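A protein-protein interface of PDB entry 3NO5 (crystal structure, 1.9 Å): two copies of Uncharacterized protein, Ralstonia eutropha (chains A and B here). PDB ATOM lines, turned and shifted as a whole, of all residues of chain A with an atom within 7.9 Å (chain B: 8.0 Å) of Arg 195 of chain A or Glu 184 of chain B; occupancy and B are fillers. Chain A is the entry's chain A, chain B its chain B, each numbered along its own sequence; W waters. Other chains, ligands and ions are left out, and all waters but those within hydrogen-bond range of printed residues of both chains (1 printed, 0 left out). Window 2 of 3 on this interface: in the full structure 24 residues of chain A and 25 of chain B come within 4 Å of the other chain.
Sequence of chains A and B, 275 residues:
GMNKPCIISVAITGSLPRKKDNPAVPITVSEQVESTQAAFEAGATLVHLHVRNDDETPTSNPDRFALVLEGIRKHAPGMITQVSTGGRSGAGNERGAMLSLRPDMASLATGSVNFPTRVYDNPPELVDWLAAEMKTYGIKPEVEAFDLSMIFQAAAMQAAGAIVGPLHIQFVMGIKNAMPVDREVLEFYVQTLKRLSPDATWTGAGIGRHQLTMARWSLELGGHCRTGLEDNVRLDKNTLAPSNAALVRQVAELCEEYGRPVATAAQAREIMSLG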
ATOM      1  N   LEU A 148       1.816 -10.581   4.668  1.00  0.00           N
ATOM      2  CA  LEU A 148       3.205 -10.533   4.187  1.00  0.00           C
ATOM      3  C   LEU A 148       3.953 -11.886   4.238  1.00  0.00           C
ATOM      4  O   LEU A 148       4.609 -12.250   3.259  1.00  0.00           O
ATOM      5  CB  LEU A 148       3.998  -9.437   4.934  1.00  0.00           C
ATOM      6  CG  LEU A 148       5.435  -9.179   4.447  1.00  0.00           C
ATOM      7  CD1 LEU A 148       5.462  -8.774   2.972  1.00  0.00           C
ATOM      8  CD2 LEU A 148       6.114  -8.126   5.297  1.00  0.00           C
ATOM      9  N   PHE A 152       6.708 -14.902   1.626  1.00  0.00           N
ATOM     10  CA  PHE A 152       7.932 -15.612   2.019  1.00  0.00           C
ATOM     11  C   PHE A 152       7.738 -17.117   1.984  1.00  0.00           C
ATOM     12  O   PHE A 152       8.620 -17.832   1.515  1.00  0.00           O
ATOM     13  CB  PHE A 152       8.401 -15.160   3.407  1.00  0.00           C
ATOM     14  CG  PHE A 152       9.057 -13.806   3.392  1.00  0.00           C
ATOM     15  CD1 PHE A 152      10.423 -13.682   3.166  1.00  0.00           C
ATOM     16  CD2 PHE A 152       8.303 -12.649   3.530  1.00  0.00           C
ATOM     17  CE1 PHE A 152      11.025 -12.426   3.109  1.00  0.00           C
ATOM     18  CE2 PHE A 152       8.907 -11.395   3.467  1.00  0.00           C
ATOM     19  CZ  PHE A 152      10.265 -11.292   3.248  1.00  0.00           C
ATOM     20  N   ALA A 155       7.679 -18.299  -1.714  1.00  0.00           N
ATOM     21  CA  ALA A 155       9.040 -18.288  -2.256  1.00  0.00           C
ATOM     22  C   ALA A 155       9.871 -19.451  -1.716  1.00  0.00           C
ATOM     23  O   ALA A 155      10.631 -20.055  -2.468  1.00  0.00           O
ATOM     24  CB  ALA A 155       9.719 -16.966  -1.935  1.00  0.00           C
ATOM     25  N   PHE A 188       5.400  -2.556  -1.280  1.00  0.00           N
ATOM     26  CA  PHE A 188       6.366  -3.395  -0.575  1.00  0.00           C
ATOM     27  C   PHE A 188       6.177  -4.870  -0.946  1.00  0.00           C
ATOM     28  O   PHE A 188       7.157  -5.587  -1.093  1.00  0.00           O
ATOM     29  CB  PHE A 188       6.269  -3.194   0.948  1.00  0.00           C
ATOM     30  CG  PHE A 188       7.345  -3.916   1.724  1.00  0.00           C
ATOM     31  CD1 PHE A 188       8.659  -3.457   1.716  1.00  0.00           C
ATOM     32  CD2 PHE A 188       7.052  -5.068   2.445  1.00  0.00           C
ATOM     33  CE1 PHE A 188       9.663  -4.147   2.402  1.00  0.00           C
ATOM     34  CE2 PHE A 188       8.051  -5.745   3.148  1.00  0.00           C
ATOM     35  CZ  PHE A 188       9.351  -5.281   3.120  1.00  0.00           C
ATOM     36  N   TYR A 189       4.903  -5.306  -1.140  1.00  0.00           N
ATOM     37  CA  TYR A 189       4.563  -6.665  -1.589  1.00  0.00           C
ATOM     38  C   TYR A 189       5.275  -6.962  -2.926  1.00  0.00           C
ATOM     39  O   TYR A 189       5.908  -8.010  -3.074  1.00  0.00           O
ATOM     40  CB  TYR A 189       3.035  -6.786  -1.803  1.00  0.00           C
ATOM     41  CG  TYR A 189       2.216  -7.150  -0.579  1.00  0.00           C
ATOM     42  CD1 TYR A 189       2.821  -7.342   0.661  1.00  0.00           C
ATOM     43  CD2 TYR A 189       0.842  -7.344  -0.670  1.00  0.00           C
ATOM     44  CE1 TYR A 189       2.080  -7.743   1.773  1.00  0.00           C
ATOM     45  CE2 TYR A 189       0.092  -7.749   0.431  1.00  0.00           C
ATOM     46  CZ  TYR A 189       0.712  -7.941   1.653  1.00  0.00           C
ATOM     47  OH  TYR A 189      -0.035  -8.339   2.734  1.00  0.00           O
ATOM     48  N   VAL A 190       5.143  -6.034  -3.905  1.00  0.00           N
ATOM     49  CA  VAL A 190       5.733  -6.170  -5.247  1.00  0.00           C
ATOM     50  C   VAL A 190       7.271  -6.181  -5.174  1.00  0.00           C
ATOM     51  O   VAL A 190       7.908  -7.029  -5.801  1.00  0.00           O
ATOM     52  CB  VAL A 190       5.205  -5.060  -6.210  1.00  0.00           C
ATOM     53  CG1 VAL A 190       5.810  -5.201  -7.607  1.00  0.00           C
ATOM     54  CG2 VAL A 190       3.681  -5.084  -6.279  1.00  0.00           C
ATOM     55  N   GLN A 191       7.859  -5.257  -4.378  1.00  0.00           N
ATOM     56  CA  GLN A 191       9.315  -5.181  -4.176  1.00  0.00           C
ATOM     57  C   GLN A 191       9.846  -6.468  -3.527  1.00  0.00           C
ATOM     58  O   GLN A 191      10.895  -6.970  -3.927  1.00  0.00           O
ATOM     59  CB  GLN A 191       9.675  -3.965  -3.310  1.00  0.00           C
ATOM     60  CG  GLN A 191       9.530  -2.624  -4.027  1.00  0.00           C
ATOM     61  CD  GLN A 191       9.640  -1.456  -3.072  1.00  0.00           C
ATOM     62  OE1 GLN A 191      10.096  -1.587  -1.926  1.00  0.00           O
ATOM     63  NE2 GLN A 191       9.228  -0.281  -3.528  1.00  0.00           N
ATOM     64  N   THR A 192       9.109  -7.006  -2.533  1.00  0.00           N
ATOM     65  CA  THR A 192       9.486  -8.243  -1.839  1.00  0.00           C
ATOM     66  C   THR A 192       9.401  -9.447  -2.788  1.00  0.00           C
ATOM     67  O   THR A 192      10.320 -10.269  -2.820  1.00  0.00           O
ATOM     68  CB  THR A 192       8.617  -8.437  -0.582  1.00  0.00           C
ATOM     69  OG1 THR A 192       8.745  -7.286   0.251  1.00  0.00           O
ATOM     70  CG2 THR A 192       8.994  -9.689   0.204  1.00  0.00           C
ATOM     71  N   LEU A 193       8.303  -9.539  -3.572  1.00  0.00           N
ATOM     72  CA  LEU A 193       8.128 -10.617  -4.547  1.00  0.00           C
ATOM     73  C   LEU A 193       9.248 -10.592  -5.586  1.00  0.00           C
ATOM     74  O   LEU A 193       9.782 -11.640  -5.929  1.00  0.00           O
ATOM     75  CB  LEU A 193       6.753 -10.505  -5.236  1.00  0.00           C
ATOM     76  CG  LEU A 193       6.452 -11.560  -6.307  1.00  0.00           C
ATOM     77  CD1 LEU A 193       6.215 -12.935  -5.676  1.00  0.00           C
ATOM     78  CD2 LEU A 193       5.268 -11.145  -7.167  1.00  0.00           C
ATOM     79  N   LYS A 194       9.623  -9.386  -6.060  1.00  0.00           N
ATOM     80  CA  LYS A 194      10.701  -9.209  -7.047  1.00  0.00           C
ATOM     81  C   LYS A 194      12.055  -9.668  -6.473  1.00  0.00           C
ATOM     82  O   LYS A 194      12.848 -10.286  -7.183  1.00  0.00           O
ATOM     83  CB  LYS A 194      10.773  -7.736  -7.504  1.00  0.00           C
ATOM     84  CG  LYS A 194      11.701  -7.493  -8.691  1.00  0.00           C
ATOM     85  CD  LYS A 194      11.853  -6.002  -8.976  1.00  0.00           C
ATOM     86  CE  LYS A 194      13.075  -5.685  -9.814  1.00  0.00           C
ATOM     87  NZ  LYS A 194      12.933  -6.163 -11.217  1.00  0.00           N
ATOM     88  N   ARG A 195      12.293  -9.399  -5.182  1.00  0.00           N
ATOM     89  CA  ARG A 195      13.535  -9.779  -4.499  1.00  0.00           C
ATOM     90  C   ARG A 195      13.630 -11.313  -4.313  1.00  0.00           C
ATOM     91  O   ARG A 195      14.687 -11.898  -4.550  1.00  0.00           O
ATOM     92  CB  ARG A 195      13.635  -9.053  -3.138  1.00  0.00           C
ATOM     93  CG  ARG A 195      14.818  -9.491  -2.272  1.00  0.00           C
ATOM     94  CD  ARG A 195      15.105  -8.506  -1.145  1.00  0.00           C
ATOM     95  NE  ARG A 195      13.962  -8.333  -0.238  1.00  0.00           N
ATOM     96  CZ  ARG A 195      13.809  -9.001   0.902  1.00  0.00           C
ATOM     97  NH1 ARG A 195      14.698  -9.916   1.267  1.00  0.00           N
ATOM     98  NH2 ARG A 195      12.759  -8.768   1.678  1.00  0.00           N
ATOM     99  N   LEU A 196      12.520 -11.951  -3.905  1.00  0.00           N
ATOM    100  CA  LEU A 196      12.490 -13.393  -3.625  1.00  0.00           C
ATOM    101  C   LEU A 196      12.292 -14.247  -4.886  1.00  0.00           C
ATOM    102  O   LEU A 196      12.862 -15.331  -4.982  1.00  0.00           O
ATOM    103  CB  LEU A 196      11.383 -13.719  -2.601  1.00  0.00           C
ATOM    104  CG  LEU A 196      11.471 -13.022  -1.229  1.00  0.00           C
ATOM    105  CD1 LEU A 196      10.187 -13.220  -0.445  1.00  0.00           C
ATOM    106  CD2 LEU A 196      12.673 -13.527  -0.420  1.00  0.00           C
ATOM    107  N   SER A 197      11.411 -13.802  -5.802  1.00  0.00           N
ATOM    108  CA  SER A 197      11.049 -14.565  -7.007  1.00  0.00           C
ATOM    109  C   SER A 197      10.980 -13.603  -8.224  1.00  0.00           C
ATOM    110  O   SER A 197       9.909 -13.087  -8.545  1.00  0.00           O
ATOM    111  CB  SER A 197       9.701 -15.260  -6.796  1.00  0.00           C
ATOM    112  OG  SER A 197       9.511 -16.334  -7.697  1.00  0.00           O
ATOM    113  N   PRO A 198      12.145 -13.315  -8.879  1.00  0.00           N
ATOM    114  CA  PRO A 198      12.165 -12.256  -9.918  1.00  0.00           C
ATOM    115  C   PRO A 198      11.272 -12.488 -11.139  1.00  0.00           C
ATOM    116  O   PRO A 198      10.868 -11.517 -11.778  1.00  0.00           O
ATOM    117  CB  PRO A 198      13.646 -12.169 -10.310  1.00  0.00           C
ATOM    118  CG  PRO A 198      14.385 -12.752  -9.162  1.00  0.00           C
ATOM    119  CD  PRO A 198      13.507 -13.799  -8.574  1.00  0.00           C
ATOM    120  N   ASP A 199      11.000 -13.757 -11.494  1.00  0.00           N
ATOM    121  CA  ASP A 199      10.191 -14.076 -12.681  1.00  0.00           C
ATOM    122  C   ASP A 199       8.705 -14.280 -12.352  1.00  0.00           C
ATOM    123  O   ASP A 199       7.926 -14.668 -13.231  1.00  0.00           O
ATOM    124  CB  ASP A 199      10.767 -15.302 -13.422  1.00  0.00           C
ATOM    125  CG  ASP A 199      10.782 -16.589 -12.605  1.00  0.00           C
ATOM    126  OD1 ASP A 199      10.843 -16.501 -11.354  1.00  0.00           O
ATOM    127  OD2 ASP A 199      10.797 -17.672 -13.213  1.00  0.00           O
ATOM    128  N   MET B 173      10.574 -12.503  14.799  1.00  0.00           N
ATOM    129  CA  MET B 173      11.158 -13.126  13.599  1.00  0.00           C
ATOM    130  C   MET B 173      11.912 -14.429  13.911  1.00  0.00           C
ATOM    131  O   MET B 173      12.484 -14.575  14.992  1.00  0.00           O
ATOM    132  CB  MET B 173      12.089 -12.145  12.868  1.00  0.00           C
ATOM    133  CG  MET B 173      11.359 -11.003  12.208  1.00  0.00           C
ATOM    134  SD  MET B 173      12.542  -9.779  11.297  1.00  0.00           S
ATOM    135  CE  MET B 173      11.285  -8.739  10.555  1.00  0.00           C
ATOM    136  N   VAL B 181      13.597 -14.225   9.590  1.00  0.00           N
ATOM    137  CA  VAL B 181      14.477 -13.099   9.891  1.00  0.00           C
ATOM    138  C   VAL B 181      14.819 -12.357   8.594  1.00  0.00           C
ATOM    139  O   VAL B 181      15.270 -12.978   7.627  1.00  0.00           O
ATOM    140  CB  VAL B 181      15.746 -13.538  10.691  1.00  0.00           C
ATOM    141  CG1 VAL B 181      16.636 -14.471   9.868  1.00  0.00           C
ATOM    142  CG2 VAL B 181      16.531 -12.331  11.185  1.00  0.00           C
ATOM    143  N   ASP B 182      14.446 -11.070   8.519  1.00  0.00           N
ATOM    144  CA  ASP B 182      14.692 -10.265   7.328  1.00  0.00           C
ATOM    145  C   ASP B 182      14.834  -8.792   7.700  1.00  0.00           C
ATOM    146  O   ASP B 182      13.934  -8.213   8.314  1.00  0.00           O
ATOM    147  CB  ASP B 182      13.571 -10.474   6.280  1.00  0.00           C
ATOM    148  CG  ASP B 182      13.862  -9.838   4.933  1.00  0.00           C
ATOM    149  OD1 ASP B 182      13.493  -8.670   4.742  1.00  0.00           O
ATOM    150  OD2 ASP B 182      14.425 -10.526   4.065  1.00  0.00           O
ATOM    151  N   ARG B 183      15.986  -8.202   7.370  1.00  0.00           N
ATOM    152  CA  ARG B 183      16.302  -6.807   7.676  1.00  0.00           C
ATOM    153  C   ARG B 183      15.331  -5.822   7.006  1.00  0.00           C
ATOM    154  O   ARG B 183      14.856  -4.891   7.662  1.00  0.00           O
ATOM    155  CB  ARG B 183      17.767  -6.491   7.280  1.00  0.00           C
ATOM    156  CG  ARG B 183      18.152  -5.012   7.387  1.00  0.00           C
ATOM    157  CD  ARG B 183      18.511  -4.600   8.801  1.00  0.00           C
ATOM    158  NE  ARG B 183      18.930  -3.199   8.859  1.00  0.00           N
ATOM    159  CZ  ARG B 183      19.495  -2.636   9.920  1.00  0.00           C
ATOM    160  NH1 ARG B 183      19.726  -3.350  11.014  1.00  0.00           N
ATOM    161  NH2 ARG B 183      19.848  -1.358   9.891  1.00  0.00           N
ATOM    162  N   GLU B 184      15.043  -6.024   5.699  1.00  0.00           N
ATOM    163  CA  GLU B 184      14.169  -5.129   4.942  1.00  0.00           C
ATOM    164  C   GLU B 184      12.738  -5.122   5.475  1.00  0.00           C
ATOM    165  O   GLU B 184      12.115  -4.059   5.530  1.00  0.00           O
ATOM    166  CB  GLU B 184      14.214  -5.457   3.442  1.00  0.00           C
ATOM    167  CG  GLU B 184      15.567  -5.154   2.818  1.00  0.00           C
ATOM    168  CD  GLU B 184      15.786  -5.764   1.451  1.00  0.00           C
ATOM    169  OE1 GLU B 184      16.469  -6.810   1.371  1.00  0.00           O
ATOM    170  OE2 GLU B 184      15.311  -5.175   0.454  1.00  0.00           O
ATOM    171  N   VAL B 185      12.217  -6.303   5.913  1.00  0.00           N
ATOM    172  CA  VAL B 185      10.873  -6.406   6.513  1.00  0.00           C
ATOM    173  C   VAL B 185      10.836  -5.650   7.850  1.00  0.00           C
ATOM    174  O   VAL B 185       9.893  -4.912   8.122  1.00  0.00           O
ATOM    175  CB  VAL B 185      10.437  -7.894   6.682  1.00  0.00           C
ATOM    176  CG1 VAL B 185       9.222  -8.018   7.602  1.00  0.00           C
ATOM    177  CG2 VAL B 185      10.157  -8.531   5.335  1.00  0.00           C
ATOM    178  N   LEU B 186      11.903  -5.822   8.684  1.00  0.00           N
ATOM    179  CA  LEU B 186      11.974  -5.133   9.981  1.00  0.00           C
ATOM    180  C   LEU B 186      11.992  -3.625   9.776  1.00  0.00           C
ATOM    181  O   LEU B 186      11.282  -2.908  10.471  1.00  0.00           O
ATOM    182  CB  LEU B 186      13.208  -5.586  10.793  1.00  0.00           C
ATOM    183  CG  LEU B 186      13.363  -4.945  12.191  1.00  0.00           C
ATOM    184  CD1 LEU B 186      12.150  -5.244  13.081  1.00  0.00           C
ATOM    185  CD2 LEU B 186      14.622  -5.417  12.865  1.00  0.00           C
ATOM    186  N   GLU B 187      12.766  -3.145   8.776  1.00  0.00           N
ATOM    187  CA  GLU B 187      12.812  -1.718   8.438  1.00  0.00           C
ATOM    188  C   GLU B 187      11.437  -1.225   7.990  1.00  0.00           C
ATOM    189  O   GLU B 187      11.003  -0.150   8.414  1.00  0.00           O
ATOM    190  CB  GLU B 187      13.864  -1.448   7.361  1.00  0.00           C
ATOM    191  CG  GLU B 187      15.290  -1.569   7.873  1.00  0.00           C
ATOM    192  CD  GLU B 187      16.368  -1.304   6.837  1.00  0.00           C
ATOM    193  OE1 GLU B 187      16.025  -0.880   5.710  1.00  0.00           O
ATOM    194  OE2 GLU B 187      17.561  -1.506   7.160  1.00  0.00           O
ATOM    195  N   PHE B 188      10.712  -2.050   7.191  1.00  0.00           N
ATOM    196  CA  PHE B 188       9.362  -1.702   6.747  1.00  0.00           C
ATOM    197  C   PHE B 188       8.378  -1.717   7.924  1.00  0.00           C
ATOM    198  O   PHE B 188       7.495  -0.864   7.992  1.00  0.00           O
ATOM    199  CB  PHE B 188       8.891  -2.632   5.623  1.00  0.00           C
ATOM    200  CG  PHE B 188       7.563  -2.231   5.022  1.00  0.00           C
ATOM    201  CD1 PHE B 188       7.463  -1.119   4.184  1.00  0.00           C
ATOM    202  CD2 PHE B 188       6.407  -2.955   5.300  1.00  0.00           C
ATOM    203  CE1 PHE B 188       6.228  -0.736   3.649  1.00  0.00           C
ATOM    204  CE2 PHE B 188       5.175  -2.574   4.755  1.00  0.00           C
ATOM    205  CZ  PHE B 188       5.093  -1.467   3.937  1.00  0.00           C
ATOM    206  N   TYR B 189       8.561  -2.675   8.875  1.00  0.00           N
ATOM    207  CA  TYR B 189       7.767  -2.756  10.114  1.00  0.00           C
ATOM    208  C   TYR B 189       7.854  -1.422  10.877  1.00  0.00           C
ATOM    209  O   TYR B 189       6.829  -0.873  11.287  1.00  0.00           O
ATOM    210  CB  TYR B 189       8.312  -3.889  11.022  1.00  0.00           C
ATOM    211  CG  TYR B 189       7.767  -5.282  10.751  1.00  0.00           C
ATOM    212  CD1 TYR B 189       6.843  -5.509   9.735  1.00  0.00           C
ATOM    213  CD2 TYR B 189       8.148  -6.364  11.540  1.00  0.00           C
ATOM    214  CE1 TYR B 189       6.291  -6.776   9.528  1.00  0.00           C
ATOM    215  CE2 TYR B 189       7.610  -7.633  11.338  1.00  0.00           C
ATOM    216  CZ  TYR B 189       6.686  -7.837  10.328  1.00  0.00           C
ATOM    217  OH  TYR B 189       6.157  -9.091  10.133  1.00  0.00           O
ATOM    218  N   VAL B 190       9.098  -0.921  11.090  1.00  0.00           N
ATOM    219  CA  VAL B 190       9.365   0.328  11.821  1.00  0.00           C
ATOM    220  C   VAL B 190       8.767   1.541  11.085  1.00  0.00           C
ATOM    221  O   VAL B 190       8.130   2.387  11.716  1.00  0.00           O
ATOM    222  CB  VAL B 190      10.887   0.504  12.098  1.00  0.00           C
ATOM    223  CG1 VAL B 190      11.163   1.790  12.875  1.00  0.00           C
ATOM    224  CG2 VAL B 190      11.448  -0.703  12.840  1.00  0.00           C
ATOM    225  N   GLN B 191       8.960   1.603   9.743  1.00  0.00           N
ATOM    226  CA  GLN B 191       8.419   2.674   8.900  1.00  0.00           C
ATOM    227  C   GLN B 191       6.885   2.683   8.966  1.00  0.00           C
ATOM    228  O   GLN B 191       6.276   3.757   9.039  1.00  0.00           O
ATOM    229  CB  GLN B 191       8.891   2.492   7.443  1.00  0.00           C
ATOM    230  CG  GLN B 191       8.472   3.625   6.504  1.00  0.00           C
ATOM    231  CD  GLN B 191       8.716   3.266   5.059  1.00  0.00           C
ATOM    232  OE1 GLN B 191       9.854   3.232   4.585  1.00  0.00           O
ATOM    233  NE2 GLN B 191       7.646   2.990   4.328  1.00  0.00           N
ATOM    234  N   TRP B 217      19.879  -5.481  15.433  1.00  0.00           N
ATOM    235  CA  TRP B 217      19.045  -4.667  14.549  1.00  0.00           C
ATOM    236  C   TRP B 217      18.168  -3.690  15.323  1.00  0.00           C
ATOM    237  O   TRP B 217      18.004  -2.550  14.889  1.00  0.00           O
ATOM    238  CB  TRP B 217      18.192  -5.555  13.632  1.00  0.00           C
ATOM    239  CG  TRP B 217      18.984  -6.337  12.618  1.00  0.00           C
ATOM    240  CD1 TRP B 217      20.319  -6.218  12.341  1.00  0.00           C
ATOM    241  CD2 TRP B 217      18.476  -7.334  11.725  1.00  0.00           C
ATOM    242  NE1 TRP B 217      20.675  -7.096  11.346  1.00  0.00           N
ATOM    243  CE2 TRP B 217      19.562  -7.792  10.944  1.00  0.00           C
ATOM    244  CE3 TRP B 217      17.205  -7.892  11.508  1.00  0.00           C
ATOM    245  CZ2 TRP B 217      19.415  -8.777   9.962  1.00  0.00           C
ATOM    246  CZ3 TRP B 217      17.062  -8.866  10.534  1.00  0.00           C
ATOM    247  CH2 TRP B 217      18.157  -9.300   9.775  1.00  0.00           C
ATOM    248  N   LEU B 221      18.182   0.380  14.904  1.00  0.00           N
ATOM    249  CA  LEU B 221      16.979   1.044  14.390  1.00  0.00           C
ATOM    250  C   LEU B 221      16.207   1.876  15.438  1.00  0.00           C
ATOM    251  O   LEU B 221      15.176   2.469  15.112  1.00  0.00           O
ATOM    252  CB  LEU B 221      16.052   0.018  13.696  1.00  0.00           C
ATOM    253  CG  LEU B 221      16.637  -0.656  12.433  1.00  0.00           C
ATOM    254  CD1 LEU B 221      15.842  -1.873  12.050  1.00  0.00           C
ATOM    255  CD2 LEU B 221      16.716   0.332  11.259  1.00  0.00           C
HETATM  256  O   HOH W   1      13.808  -5.380  -1.709  1.00  0.00           O
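The guanidinium group of Arg 195 of chain A lies within salt-bridge range of the side-chain carboxylate of Glu 184 of chain B, at 3.3 Å.
The side-chain carboxylate (OD2) of Asp 182 of chain B lies within salt-bridge range of the guanidinium group (NH1) of Arg 195 of chain A (2.9 Å).
The side-chain hydroxyl (OH) of Tyr 189 of chain A is in hydrogen-bond range of the backbone NH (N) of Leu 148 of chain A (3.5 Å).
O of Phe 188 of chain A lies within hydrogen-bond range of OG1 of Thr 192 of chain A (2.7 Å).
The side-chain carboxylate (OD1) of Asp 182 of chain B sits at hydrogen-bond distance from the backbone NH (N) of Val 185 of chain B, 2.9 Å away.
The side-chain sulfur of Met 173 of chain B is in hydrogen-bond range of the backbone NH of Asp 182 of chain B, at 3.6 Å.
OD1 of Asp 182 of chain B lies within hydrogen-bond range of N of Glu 184 of chain B.
Leu 148 of chain A touches Val 185 of chain B (CD2 to CG1, 3.9 Å).
Val 185 of chain B touches Phe 152 of chain A (CG2 to CZ, 3.5 Å).
Phe 188 of chain A touches Glu 184 of chain B (CZ to O, 3.9 Å).
Val 185 of chain B touches Phe 188 of chain A (CA to CZ, 3.9 Å).
CD1 of Phe 188 of chain B touches CD1 of Phe 188 of chain A, 3.6 Å away.
Printed residues of chain B within 4 Å of Leu 148 of chain A: Val 185.
Of the printed residues of chain B, Phe 152 of chain A touches Val 185.
Of the printed residues of chain B, Phe 188 of chain A touches Glu 184 (3.9 Å), Val 185 (3.9 Å) and Phe 188 (3.6 Å).
Of the printed residues of chain B, Arg 195 of chain A touches Asp 182 and Glu 184.
Arg 183 of chain B touches none of the printed residues of chain A.
Of the printed residues of chain A, Glu 184 of chain B touches Phe 188 and Arg 195.
The nearest printed residue of chain A that does not touch Glu 184 of chain B is Gln 191 of chain A (6.5 Å).
The nearest printed residue of chain A that does not touch Val 185 of chain B is Arg 195 of chain A (4.5 Å).
Of the 14 printed residues of chain B, 4 touch a printed residue of chain A.
Printed residues of chain B that touch a printed residue of chain A: Asp 182, Glu 184, Val 185 and Phe 188.
Hydrophobic or aromatic side chains of chain B that line the printed part of chain A: Val 185 and Phe 188.
Of the 15 printed residues of chain A, 4 touch a printed residue of chain B.
Hydrophobic or aromatic side chains of chain A within 4 Å of the printed part of chain B: Leu 148, Phe 152 and Phe 188.
Among the printed residues, 7 pairs touch across the chains.
Among the printed residues, Asp or Glu carboxylates within 4 Å of a Lys or Arg side-chain nitrogen of the other chain: Arg 195 of chain A with Asp 182 of chain B (2.9 Å) and Arg 195 of chain A with Glu 184 of chain B (3.3 Å).
Phe 188 of chain A touches its own counterpart, Phe 188 of chain B.
Positions printed for both chains: 188, 189, 190 and 191.
Of the 7 pairs that touch across the chains among the printed residues, 1 has its exchanged pair printed and touching as well.
Water W1 lies within hydrogen-bond range of the side-chain carboxylate (OE2) of Glu 184 of chain B and the guanidinium group (NE) of Arg 195 of chain A.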
